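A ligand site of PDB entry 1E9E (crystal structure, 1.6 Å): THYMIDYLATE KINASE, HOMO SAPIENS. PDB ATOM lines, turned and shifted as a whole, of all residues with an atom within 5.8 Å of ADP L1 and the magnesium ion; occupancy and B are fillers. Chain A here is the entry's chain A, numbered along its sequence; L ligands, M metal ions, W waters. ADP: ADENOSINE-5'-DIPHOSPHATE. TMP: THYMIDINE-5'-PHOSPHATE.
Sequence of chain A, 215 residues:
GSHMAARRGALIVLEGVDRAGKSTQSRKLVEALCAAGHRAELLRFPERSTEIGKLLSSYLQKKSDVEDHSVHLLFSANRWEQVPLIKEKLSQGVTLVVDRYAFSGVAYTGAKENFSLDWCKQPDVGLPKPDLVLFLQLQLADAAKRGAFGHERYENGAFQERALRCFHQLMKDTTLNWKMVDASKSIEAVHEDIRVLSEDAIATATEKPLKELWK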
ATOM      1  N   GLY A  16     -19.702   1.888  19.021  1.00  0.00           N
ATOM      2  CA  GLY A  16     -18.736   2.989  18.982  1.00  0.00           C
ATOM      3  C   GLY A  16     -19.434   4.280  18.577  1.00  0.00           C
ATOM      4  O   GLY A  16     -20.582   4.284  18.184  1.00  0.00           O
ATOM      5  N   VAL A  17     -18.691   5.397  18.734  1.00  0.00           N
ATOM      6  CA  VAL A  17     -19.264   6.690  18.397  1.00  0.00           C
ATOM      7  C   VAL A  17     -19.458   6.842  16.893  1.00  0.00           C
ATOM      8  O   VAL A  17     -19.111   5.987  16.076  1.00  0.00           O
ATOM      9  CB  VAL A  17     -18.309   7.796  18.911  1.00  0.00           C
ATOM     10  CG1 VAL A  17     -18.187   7.712  20.421  1.00  0.00           C
ATOM     11  CG2 VAL A  17     -16.939   7.639  18.231  1.00  0.00           C
ATOM     12  N   ASP A  18     -20.002   8.001  16.488  1.00  0.00           N
ATOM     13  CA  ASP A  18     -20.164   8.288  15.075  1.00  0.00           C
ATOM     14  C   ASP A  18     -18.806   8.295  14.392  1.00  0.00           C
ATOM     15  O   ASP A  18     -17.832   8.806  14.934  1.00  0.00           O
ATOM     16  CB  ASP A  18     -20.847   9.660  14.958  1.00  0.00           C
ATOM     17  CG  ASP A  18     -20.753  10.231  13.556  1.00  0.00           C
ATOM     18  OD1 ASP A  18     -21.491   9.702  12.703  1.00  0.00           O
ATOM     19  OD2 ASP A  18     -19.948  11.163  13.401  1.00  0.00           O
ATOM     20  N   ARG A  19     -18.740   7.670  13.228  1.00  0.00           N
ATOM     21  CA  ARG A  19     -17.553   7.622  12.390  1.00  0.00           C
ATOM     22  C   ARG A  19     -16.452   6.746  12.943  1.00  0.00           C
ATOM     23  O   ARG A  19     -15.305   6.836  12.522  1.00  0.00           O
ATOM     24  CB  ARG A  19     -17.036   9.032  12.030  1.00  0.00           C
ATOM     25  CG  ARG A  19     -18.029   9.695  11.076  1.00  0.00           C
ATOM     26  CD  ARG A  19     -17.561  11.066  10.601  1.00  0.00           C
ATOM     27  NE  ARG A  19     -17.714  12.039  11.697  1.00  0.00           N
ATOM     28  CZ  ARG A  19     -17.179  13.253  11.641  1.00  0.00           C
ATOM     29  NH1 ARG A  19     -16.465  13.652  10.603  1.00  0.00           N
ATOM     30  NH2 ARG A  19     -17.338  14.073  12.679  1.00  0.00           N
ATOM     31  N   ALA A  20     -16.780   5.861  13.886  1.00  0.00           N
ATOM     32  CA  ALA A  20     -15.822   4.929  14.460  1.00  0.00           C
ATOM     33  C   ALA A  20     -15.476   3.817  13.470  1.00  0.00           C
ATOM     34  O   ALA A  20     -14.459   3.142  13.715  1.00  0.00           O
ATOM     35  CB  ALA A  20     -16.351   4.295  15.741  1.00  0.00           C
ATOM     36  N   GLY A  21     -16.259   3.661  12.421  1.00  0.00           N
ATOM     37  CA  GLY A  21     -15.994   2.636  11.407  1.00  0.00           C
ATOM     38  C   GLY A  21     -16.947   1.438  11.535  1.00  0.00           C
ATOM     39  O   GLY A  21     -16.638   0.393  10.976  1.00  0.00           O
ATOM     40  N   LYS A  22     -18.011   1.570  12.328  1.00  0.00           N
ATOM     41  CA  LYS A  22     -18.891   0.424  12.517  1.00  0.00           C
ATOM     42  C   LYS A  22     -19.444  -0.185  11.255  1.00  0.00           C
ATOM     43  O   LYS A  22     -19.489  -1.410  11.071  1.00  0.00           O
ATOM     44  CB  LYS A  22     -20.064   0.894  13.412  1.00  0.00           C
ATOM     45  CG  LYS A  22     -19.576   1.329  14.782  1.00  0.00           C
ATOM     46  CD  LYS A  22     -20.711   1.752  15.690  1.00  0.00           C
ATOM     47  CE  LYS A  22     -21.598   2.836  15.101  1.00  0.00           C
ATOM     48  NZ  LYS A  22     -20.841   4.116  14.940  1.00  0.00           N
ATOM     49  N   SER A  23     -20.025   0.687  10.412  1.00  0.00           N
ATOM     50  CA  SER A  23     -20.655   0.131   9.204  1.00  0.00           C
ATOM     51  C   SER A  23     -19.631  -0.467   8.267  1.00  0.00           C
ATOM     52  O   SER A  23     -19.842  -1.571   7.741  1.00  0.00           O
ATOM     53  CB  SER A  23     -21.555   1.175   8.540  1.00  0.00           C
ATOM     54  OG  SER A  23     -22.471   1.638   9.532  1.00  0.00           O
ATOM     55  N   THR A  24     -18.468   0.186   8.125  1.00  0.00           N
ATOM     56  CA  THR A  24     -17.446  -0.377   7.230  1.00  0.00           C
ATOM     57  C   THR A  24     -16.998  -1.749   7.739  1.00  0.00           C
ATOM     58  O   THR A  24     -16.902  -2.728   7.009  1.00  0.00           O
ATOM     59  CB  THR A  24     -16.237   0.576   7.181  1.00  0.00           C
ATOM     60  OG1 THR A  24     -16.706   1.801   6.566  1.00  0.00           O
ATOM     61  CG2 THR A  24     -15.096   0.046   6.331  1.00  0.00           C
ATOM     62  N   GLN A  25     -16.708  -1.784   9.052  1.00  0.00           N
ATOM     63  CA  GLN A  25     -16.183  -3.010   9.637  1.00  0.00           C
ATOM     64  C   GLN A  25     -17.231  -4.115   9.693  1.00  0.00           C
ATOM     65  O   GLN A  25     -16.891  -5.289   9.504  1.00  0.00           O
ATOM     66  CB  GLN A  25     -15.590  -2.768  11.027  1.00  0.00           C
ATOM     67  CG  GLN A  25     -14.364  -1.817  10.971  1.00  0.00           C
ATOM     68  CD  GLN A  25     -13.272  -2.414  10.101  1.00  0.00           C
ATOM     69  OE1 GLN A  25     -13.120  -3.630   9.932  1.00  0.00           O
ATOM     70  NE2 GLN A  25     -12.404  -1.588   9.511  1.00  0.00           N
ATOM     71  N   ARG A  27     -19.635  -4.590   7.479  1.00  0.00           N
ATOM     72  CA  ARG A  27     -19.743  -5.160   6.133  1.00  0.00           C
ATOM     73  C   ARG A  27     -18.539  -6.060   5.825  1.00  0.00           C
ATOM     74  O   ARG A  27     -18.702  -7.152   5.305  1.00  0.00           O
ATOM     75  CB  ARG A  27     -19.740  -4.025   5.085  1.00  0.00           C
ATOM     76  CG  ARG A  27     -21.028  -3.231   5.058  1.00  0.00           C
ATOM     77  CD  ARG A  27     -21.036  -2.239   3.894  1.00  0.00           C
ATOM     78  NE  ARG A  27     -19.941  -1.274   3.957  1.00  0.00           N
ATOM     79  CZ  ARG A  27     -20.011  -0.059   4.476  1.00  0.00           C
ATOM     80  NH1 ARG A  27     -21.111   0.424   5.071  1.00  0.00           N
ATOM     81  NH2 ARG A  27     -18.918   0.714   4.431  1.00  0.00           N
ATOM     82  N   ASP A  99     -24.574  -4.032  13.375  1.00  0.00           N
ATOM     83  CA  ASP A  99     -24.043  -2.660  13.438  1.00  0.00           C
ATOM     84  C   ASP A  99     -24.929  -1.884  14.409  1.00  0.00           C
ATOM     85  O   ASP A  99     -26.020  -1.483  13.971  1.00  0.00           O
ATOM     86  CB  ASP A  99     -24.136  -2.123  12.010  1.00  0.00           C
ATOM     87  CG  ASP A  99     -23.625  -0.738  11.732  1.00  0.00           C
ATOM     88  OD1 ASP A  99     -23.227  -0.040  12.687  1.00  0.00           O
ATOM     89  OD2 ASP A  99     -23.654  -0.409  10.525  1.00  0.00           O
ATOM     90  N   ARG A 100     -24.503  -1.809  15.638  1.00  0.00           N
ATOM     91  CA  ARG A 100     -25.179  -1.169  16.749  1.00  0.00           C
ATOM     92  C   ARG A 100     -26.279  -2.080  17.342  1.00  0.00           C
ATOM     93  O   ARG A 100     -26.878  -2.892  16.685  1.00  0.00           O
ATOM     94  CB  ARG A 100     -25.890   0.143  16.410  1.00  0.00           C
ATOM     95  CG  ARG A 100     -24.975   1.292  15.980  1.00  0.00           C
ATOM     96  CD  ARG A 100     -25.839   2.558  15.958  1.00  0.00           C
ATOM     97  NE  ARG A 100     -25.141   3.678  15.344  1.00  0.00           N
ATOM     98  CZ  ARG A 100     -24.329   4.507  15.974  1.00  0.00           C
ATOM     99  NH1 ARG A 100     -24.033   4.450  17.264  1.00  0.00           N
ATOM    100  NH2 ARG A 100     -23.761   5.488  15.262  1.00  0.00           N
ATOM    101  N   ARG A 146     -12.541  12.358   9.900  1.00  0.00           N
ATOM    102  CA  ARG A 146     -13.105  11.528   8.848  1.00  0.00           C
ATOM    103  C   ARG A 146     -14.243  12.299   8.183  1.00  0.00           C
ATOM    104  O   ARG A 146     -15.417  11.992   8.359  1.00  0.00           O
ATOM    105  CB  ARG A 146     -13.611  10.189   9.401  1.00  0.00           C
ATOM    106  CG  ARG A 146     -12.457   9.423  10.014  1.00  0.00           C
ATOM    107  CD  ARG A 146     -12.903   8.167  10.767  1.00  0.00           C
ATOM    108  NE  ARG A 146     -11.670   7.497  11.214  1.00  0.00           N
ATOM    109  CZ  ARG A 146     -11.581   6.267  11.701  1.00  0.00           C
ATOM    110  NH1 ARG A 146     -12.685   5.548  11.865  1.00  0.00           N
ATOM    111  NH2 ARG A 146     -10.399   5.811  12.056  1.00  0.00           N
ATOM    112  N   ALA A 183      -9.722   1.498  16.774  1.00  0.00           N
ATOM    113  CA  ALA A 183     -10.335   1.884  15.505  1.00  0.00           C
ATOM    114  C   ALA A 183      -9.624   3.037  14.808  1.00  0.00           C
ATOM    115  O   ALA A 183     -10.099   3.461  13.758  1.00  0.00           O
ATOM    116  CB  ALA A 183     -11.805   2.201  15.780  1.00  0.00           C
ATOM    117  N   SER A 184      -8.513   3.478  15.379  1.00  0.00           N
ATOM    118  CA  SER A 184      -7.764   4.573  14.730  1.00  0.00           C
ATOM    119  C   SER A 184      -6.893   4.066  13.604  1.00  0.00           C
ATOM    120  O   SER A 184      -6.353   4.855  12.810  1.00  0.00           O
ATOM    121  CB  SER A 184      -6.901   5.314  15.764  1.00  0.00           C
ATOM    122  OG  SER A 184      -5.802   4.503  16.177  1.00  0.00           O
ATOM    123  N   LYS A 185      -6.666   2.754  13.546  1.00  0.00           N
ATOM    124  CA  LYS A 185      -5.812   2.204  12.494  1.00  0.00           C
ATOM    125  C   LYS A 185      -6.497   2.217  11.141  1.00  0.00           C
ATOM    126  O   LYS A 185      -7.616   2.723  10.975  1.00  0.00           O
ATOM    127  CB  LYS A 185      -5.330   0.799  12.904  1.00  0.00           C
ATOM    128  CG  LYS A 185      -4.584   0.820  14.226  1.00  0.00           C
ATOM    129  CD  LYS A 185      -3.876  -0.498  14.502  1.00  0.00           C
ATOM    130  CE  LYS A 185      -4.853  -1.595  14.891  1.00  0.00           C
ATOM    131  NZ  LYS A 185      -4.184  -2.807  15.467  1.00  0.00           N
ATOM    132  N   SER A 186      -5.834   1.605  10.136  1.00  0.00           N
ATOM    133  CA  SER A 186      -6.369   1.590   8.801  1.00  0.00           C
ATOM    134  C   SER A 186      -7.609   0.677   8.723  1.00  0.00           C
ATOM    135  O   SER A 186      -7.748  -0.176   9.597  1.00  0.00           O
ATOM    136  CB  SER A 186      -5.354   1.076   7.802  1.00  0.00           C
ATOM    137  OG  SER A 186      -5.047  -0.307   7.976  1.00  0.00           O
ATOM    138  N   ILE A 187      -8.401   0.865   7.698  1.00  0.00           N
ATOM    139  CA  ILE A 187      -9.558  -0.028   7.545  1.00  0.00           C
ATOM    140  C   ILE A 187      -9.118  -1.488   7.567  1.00  0.00           C
ATOM    141  O   ILE A 187      -9.799  -2.314   8.237  1.00  0.00           O
ATOM    142  CB  ILE A 187     -10.312   0.324   6.270  1.00  0.00           C
ATOM    143  CG1 ILE A 187     -11.067   1.656   6.462  1.00  0.00           C
ATOM    144  CG2 ILE A 187     -11.232  -0.800   5.854  1.00  0.00           C
ATOM    145  CD1 ILE A 187     -11.750   2.120   5.186  1.00  0.00           C
ATOM    146  N   VAL A 190      -7.839  -2.615  11.186  1.00  0.00           N
ATOM    147  CA  VAL A 190      -8.940  -2.742  12.142  1.00  0.00           C
ATOM    148  C   VAL A 190      -9.720  -4.014  11.814  1.00  0.00           C
ATOM    149  O   VAL A 190     -10.140  -4.754  12.680  1.00  0.00           O
ATOM    150  CB  VAL A 190      -9.847  -1.502  12.044  1.00  0.00           C
ATOM    151  CG1 VAL A 190     -11.083  -1.639  12.912  1.00  0.00           C
ATOM    152  CG2 VAL A 190      -9.058  -0.262  12.502  1.00  0.00           C
HETATM  153  PB  ADP L   1     -19.770   4.482  11.433  1.00  0.00           P
HETATM  154  O1B ADP L   1     -19.173   4.117  12.745  1.00  0.00           O
HETATM  155  O2B ADP L   1     -20.779   3.536  10.909  1.00  0.00           O
HETATM  156  O3B ADP L   1     -20.365   5.940  11.434  1.00  0.00           O
HETATM  157  PA  ADP L   1     -18.317   4.274   8.868  1.00  0.00           P
HETATM  158  O1A ADP L   1     -19.522   4.653   8.104  1.00  0.00           O
HETATM  159  O2A ADP L   1     -17.850   2.849   8.724  1.00  0.00           O
HETATM  160  O3A ADP L   1     -18.473   4.585  10.439  1.00  0.00           O
HETATM  161  O5' ADP L   1     -17.077   5.200   8.534  1.00  0.00           O
HETATM  162  C5' ADP L   1     -17.186   6.624   8.698  1.00  0.00           C
HETATM  163  C4' ADP L   1     -16.334   7.298   7.608  1.00  0.00           C
HETATM  164  O4' ADP L   1     -14.970   7.068   7.937  1.00  0.00           O
HETATM  165  C3' ADP L   1     -16.551   6.781   6.201  1.00  0.00           C
HETATM  166  O3' ADP L   1     -16.196   7.792   5.254  1.00  0.00           O
HETATM  167  C2' ADP L   1     -15.471   5.671   6.119  1.00  0.00           C
HETATM  168  O2' ADP L   1     -14.946   5.385   4.851  1.00  0.00           O
HETATM  169  C1' ADP L   1     -14.347   6.315   6.938  1.00  0.00           C
HETATM  170  N9  ADP L   1     -13.540   5.293   7.629  1.00  0.00           N
HETATM  171  C8  ADP L   1     -14.002   4.102   8.153  1.00  0.00           C
HETATM  172  N7  ADP L   1     -13.022   3.446   8.770  1.00  0.00           N
HETATM  173  C5  ADP L   1     -11.890   4.267   8.642  1.00  0.00           C
HETATM  174  C6  ADP L   1     -10.579   4.114   9.074  1.00  0.00           C
HETATM  175  N6  ADP L   1     -10.120   3.085   9.741  1.00  0.00           N
HETATM  176  N1  ADP L   1      -9.778   5.149   8.734  1.00  0.00           N
HETATM  177  C2  ADP L   1     -10.201   6.211   8.052  1.00  0.00           C
HETATM  178  N3  ADP L   1     -11.421   6.441   7.603  1.00  0.00           N
HETATM  179  C4  ADP L   1     -12.180   5.410   7.950  1.00  0.00           C
HETATM  180  P   TMP L   2     -26.140   5.028  12.534  1.00  0.00           P
HETATM  181  O1P TMP L   2     -25.009   5.986  12.886  1.00  0.00           O
HETATM  182  O2P TMP L   2     -25.709   3.640  12.820  1.00  0.00           O
HETATM  183  O3P TMP L   2     -26.660   5.317  11.102  1.00  0.00           O
HETATM  184  O5' TMP L   2     -27.326   5.318  13.539  1.00  0.00           O
HETATM  185  C5' TMP L   2     -28.177   6.485  13.488  1.00  0.00           C
HETATM  186  C4' TMP L   2     -28.291   6.975  14.944  1.00  0.00           C
HETATM  187  O4' TMP L   2     -29.171   6.284  15.830  1.00  0.00           O
HETATM  188  C3' TMP L   2     -26.987   7.199  15.657  1.00  0.00           C
HETATM  189  O3' TMP L   2     -26.875   8.554  16.027  1.00  0.00           O
HETATM  190  C2' TMP L   2     -27.122   6.375  16.952  1.00  0.00           C
HETATM  191  C1' TMP L   2     -28.637   6.320  17.115  1.00  0.00           C
HETATM  192  N1  TMP L   2     -29.247   5.300  17.960  1.00  0.00           N
HETATM  193  C2  TMP L   2     -29.998   5.693  19.073  1.00  0.00           C
HETATM  194  O2  TMP L   2     -30.130   6.828  19.488  1.00  0.00           O
HETATM  195  N3  TMP L   2     -30.584   4.605  19.688  1.00  0.00           N
HETATM  196  C4  TMP L   2     -30.449   3.311  19.241  1.00  0.00           C
HETATM  197  O4  TMP L   2     -31.078   2.286  19.913  1.00  0.00           O
HETATM  198  C5  TMP L   2     -29.624   3.002  18.041  1.00  0.00           C
HETATM  199  C5M TMP L   2     -29.505   1.609  17.569  1.00  0.00           C
HETATM  200  C6  TMP L   2     -29.069   4.080  17.444  1.00  0.00           C
HETATM  201 MG    MG M   1     -22.684   3.536  10.322  1.00  0.00          MG
HETATM  202  O   HOH W   1     -23.324   2.567  12.013  1.00  0.00           O
HETATM  203  O   HOH W   2     -20.226   6.342   5.960  1.00  0.00           O
HETATM  204  O   HOH W   3     -16.195   3.114   4.189  1.00  0.00           O
HETATM  205  O   HOH W   4     -14.197  10.077   5.826  1.00  0.00           O
HETATM  206  O   HOH W   5     -21.943   6.417  13.403  1.00  0.00           O
HETATM  207  O   HOH W   6     -12.382   1.131  10.154  1.00  0.00           O
HETATM  208  O   HOH W   7     -24.705   3.400   9.467  1.00  0.00           O
HETATM  209  O   HOH W   8      -7.231   5.413   9.899  1.00  0.00           O
HETATM  210  O   HOH W   9     -11.767   8.786   6.247  1.00  0.00           O
HETATM  211  O   HOH W  10     -12.261   2.599  12.385  1.00  0.00           O
HETATM  212  O   HOH W  11     -18.355   7.953   3.910  1.00  0.00           O
HETATM  213  O   HOH W  12     -22.088   4.464   8.529  1.00  0.00           O
HETATM  214  O   HOH W  13     -12.232   5.584   3.906  1.00  0.00           O
HETATM  215  O   HOH W  14     -20.898   7.698   9.559  1.00  0.00           O
HETATM  216  O   HOH W  15     -19.607   3.218   5.655  1.00  0.00           O
HETATM  217  O   HOH W  16     -23.128   5.429  11.196  1.00  0.00           O
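The backbone NH (N) of Arg 19 sits at hydrogen-bond distance from an oxygen (O3B) of ADP L1 (3.0 Å). A nitrogen (N1) of ADP L1 lies close to the guanidinium group (NH2) of Arg 146, at 3.4 Å. The backbone NH (N) of Gly 21 sits at hydrogen-bond distance from an oxygen (O1B) of ADP L1 (3.0 Å). N of Thr 24 lies within hydrogen-bond range of O2A of ADP L1 (2.8 Å). N of Ala 20 lies within hydrogen-bond range of O1B of ADP L1, at 3.2 Å. The guanidinium group of Arg 100 lies within salt-bridge range of an oxygen (O2P) of TMP L2 (2.6 Å). The side-chain hydroxyl of Thr 24 is in hydrogen-bond range of an oxygen (O2A) of ADP L1 (2.7 Å). The backbone NH of Lys 22 lies within hydrogen-bond range of an oxygen (O1B) of ADP L1 (2.8 Å). N of Ser 23 sits close to O2B of ADP L1 (3.0 Å). An oxygen (O1B) of ADP L1 lies within salt-bridge range of the side-chain amino group (NZ) of Lys 22 (2.8 Å). The backbone carbonyl oxygen (O) of Lys 185 lies within hydrogen-bond range of a nitrogen (N6) of ADP L1, at 2.8 Å.
The side-chain hydroxyl of Thr 24 sits at hydrogen-bond distance from the guanidinium group of Arg 27. OG of Ser 23 sits close to OD2 of Asp 99 (2.6 Å). The side-chain amino group (NZ) of Lys 22 lies within hydrogen-bond range of the backbone carbonyl oxygen (O) of Gly 16, at 3.3 Å. The backbone carbonyl oxygen (O) of Ala 183 lies within hydrogen-bond range of the guanidinium group (NH2) of Arg 146, 2.9 Å away. The side-chain carboxylate (OD2) of Asp 18 lies within salt-bridge range of the guanidinium group (NE) of Arg 19, 2.9 Å away. The side-chain amino group (NZ) of Lys 22 lies within hydrogen-bond range of the backbone carbonyl oxygen (O) of Val 17 (2.8 Å). The backbone carbonyl oxygen of Arg 146 sits at hydrogen-bond distance from the guanidinium group of Arg 19 (3.0 Å). The backbone carbonyl oxygen of Ile 187 sits at hydrogen-bond distance from the side-chain amide nitrogen of Gln 25.
N of Ile 187 lies close to N6 of ADP L1, at 3.5 Å. Val 17 touches ADP L1. C of Ser 186 touches N6 of ADP L1, 3.6 Å away. Hydrophobic or aromatic side chains within 4 Å of ADP L1: Ile 187. Within 4 Å of ADP L1: Val 17, Arg 19, Ala 20, Gly 21, Lys 22, Ser 23, Thr 24, Arg 146, Lys 185, Ser 186 and Ile 187. Along chain A the residues within 4 Å of ADP L1 span positions 17 to 187. The nearest printed residue that does not touch ADP L1 is Ala 183 (4.03 Å).
One residue has an atom within 4 Å of the magnesium ion: Ser 23. The nearest printed residue that does not touch the magnesium ion is Asp 99 (4.1 Å).
The magnesium ion is bound by an oxygen (O2B) of ADP L1 (2.0 Å), water W1 (2.1 Å), the side-chain hydroxyl of Ser 23 (2.1 Å), water W12 (2.1 Å), water W16 (2.1 Å) and water W7 (2.2 Å).
Water W16 lies within hydrogen-bond range of an oxygen (O1P) of TMP L2 (2.6 Å) and an oxygen (O3B) of ADP L1 (2.8 Å). Water W3 lies within hydrogen-bond range of O2' of ADP L1 and OG1 of Thr 24. Water W6 bridges a nitrogen (N7) of ADP L1 and the side-chain amide nitrogen of Gln 25. Water W15 lies within hydrogen-bond range of O1A of ADP L1 (2.8 Å), NH2 of Arg 27 (2.9 Å) and OG1 of Thr 24 (3.4 Å). Water W4 bridges O3' of ADP L1 (3.1 Å) and O of Arg 146 (3.4 Å). Water W10 lies within hydrogen-bond range of O of Ala 20, O of Ala 183, NH1 of Arg 146 and N6 of ADP L1.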
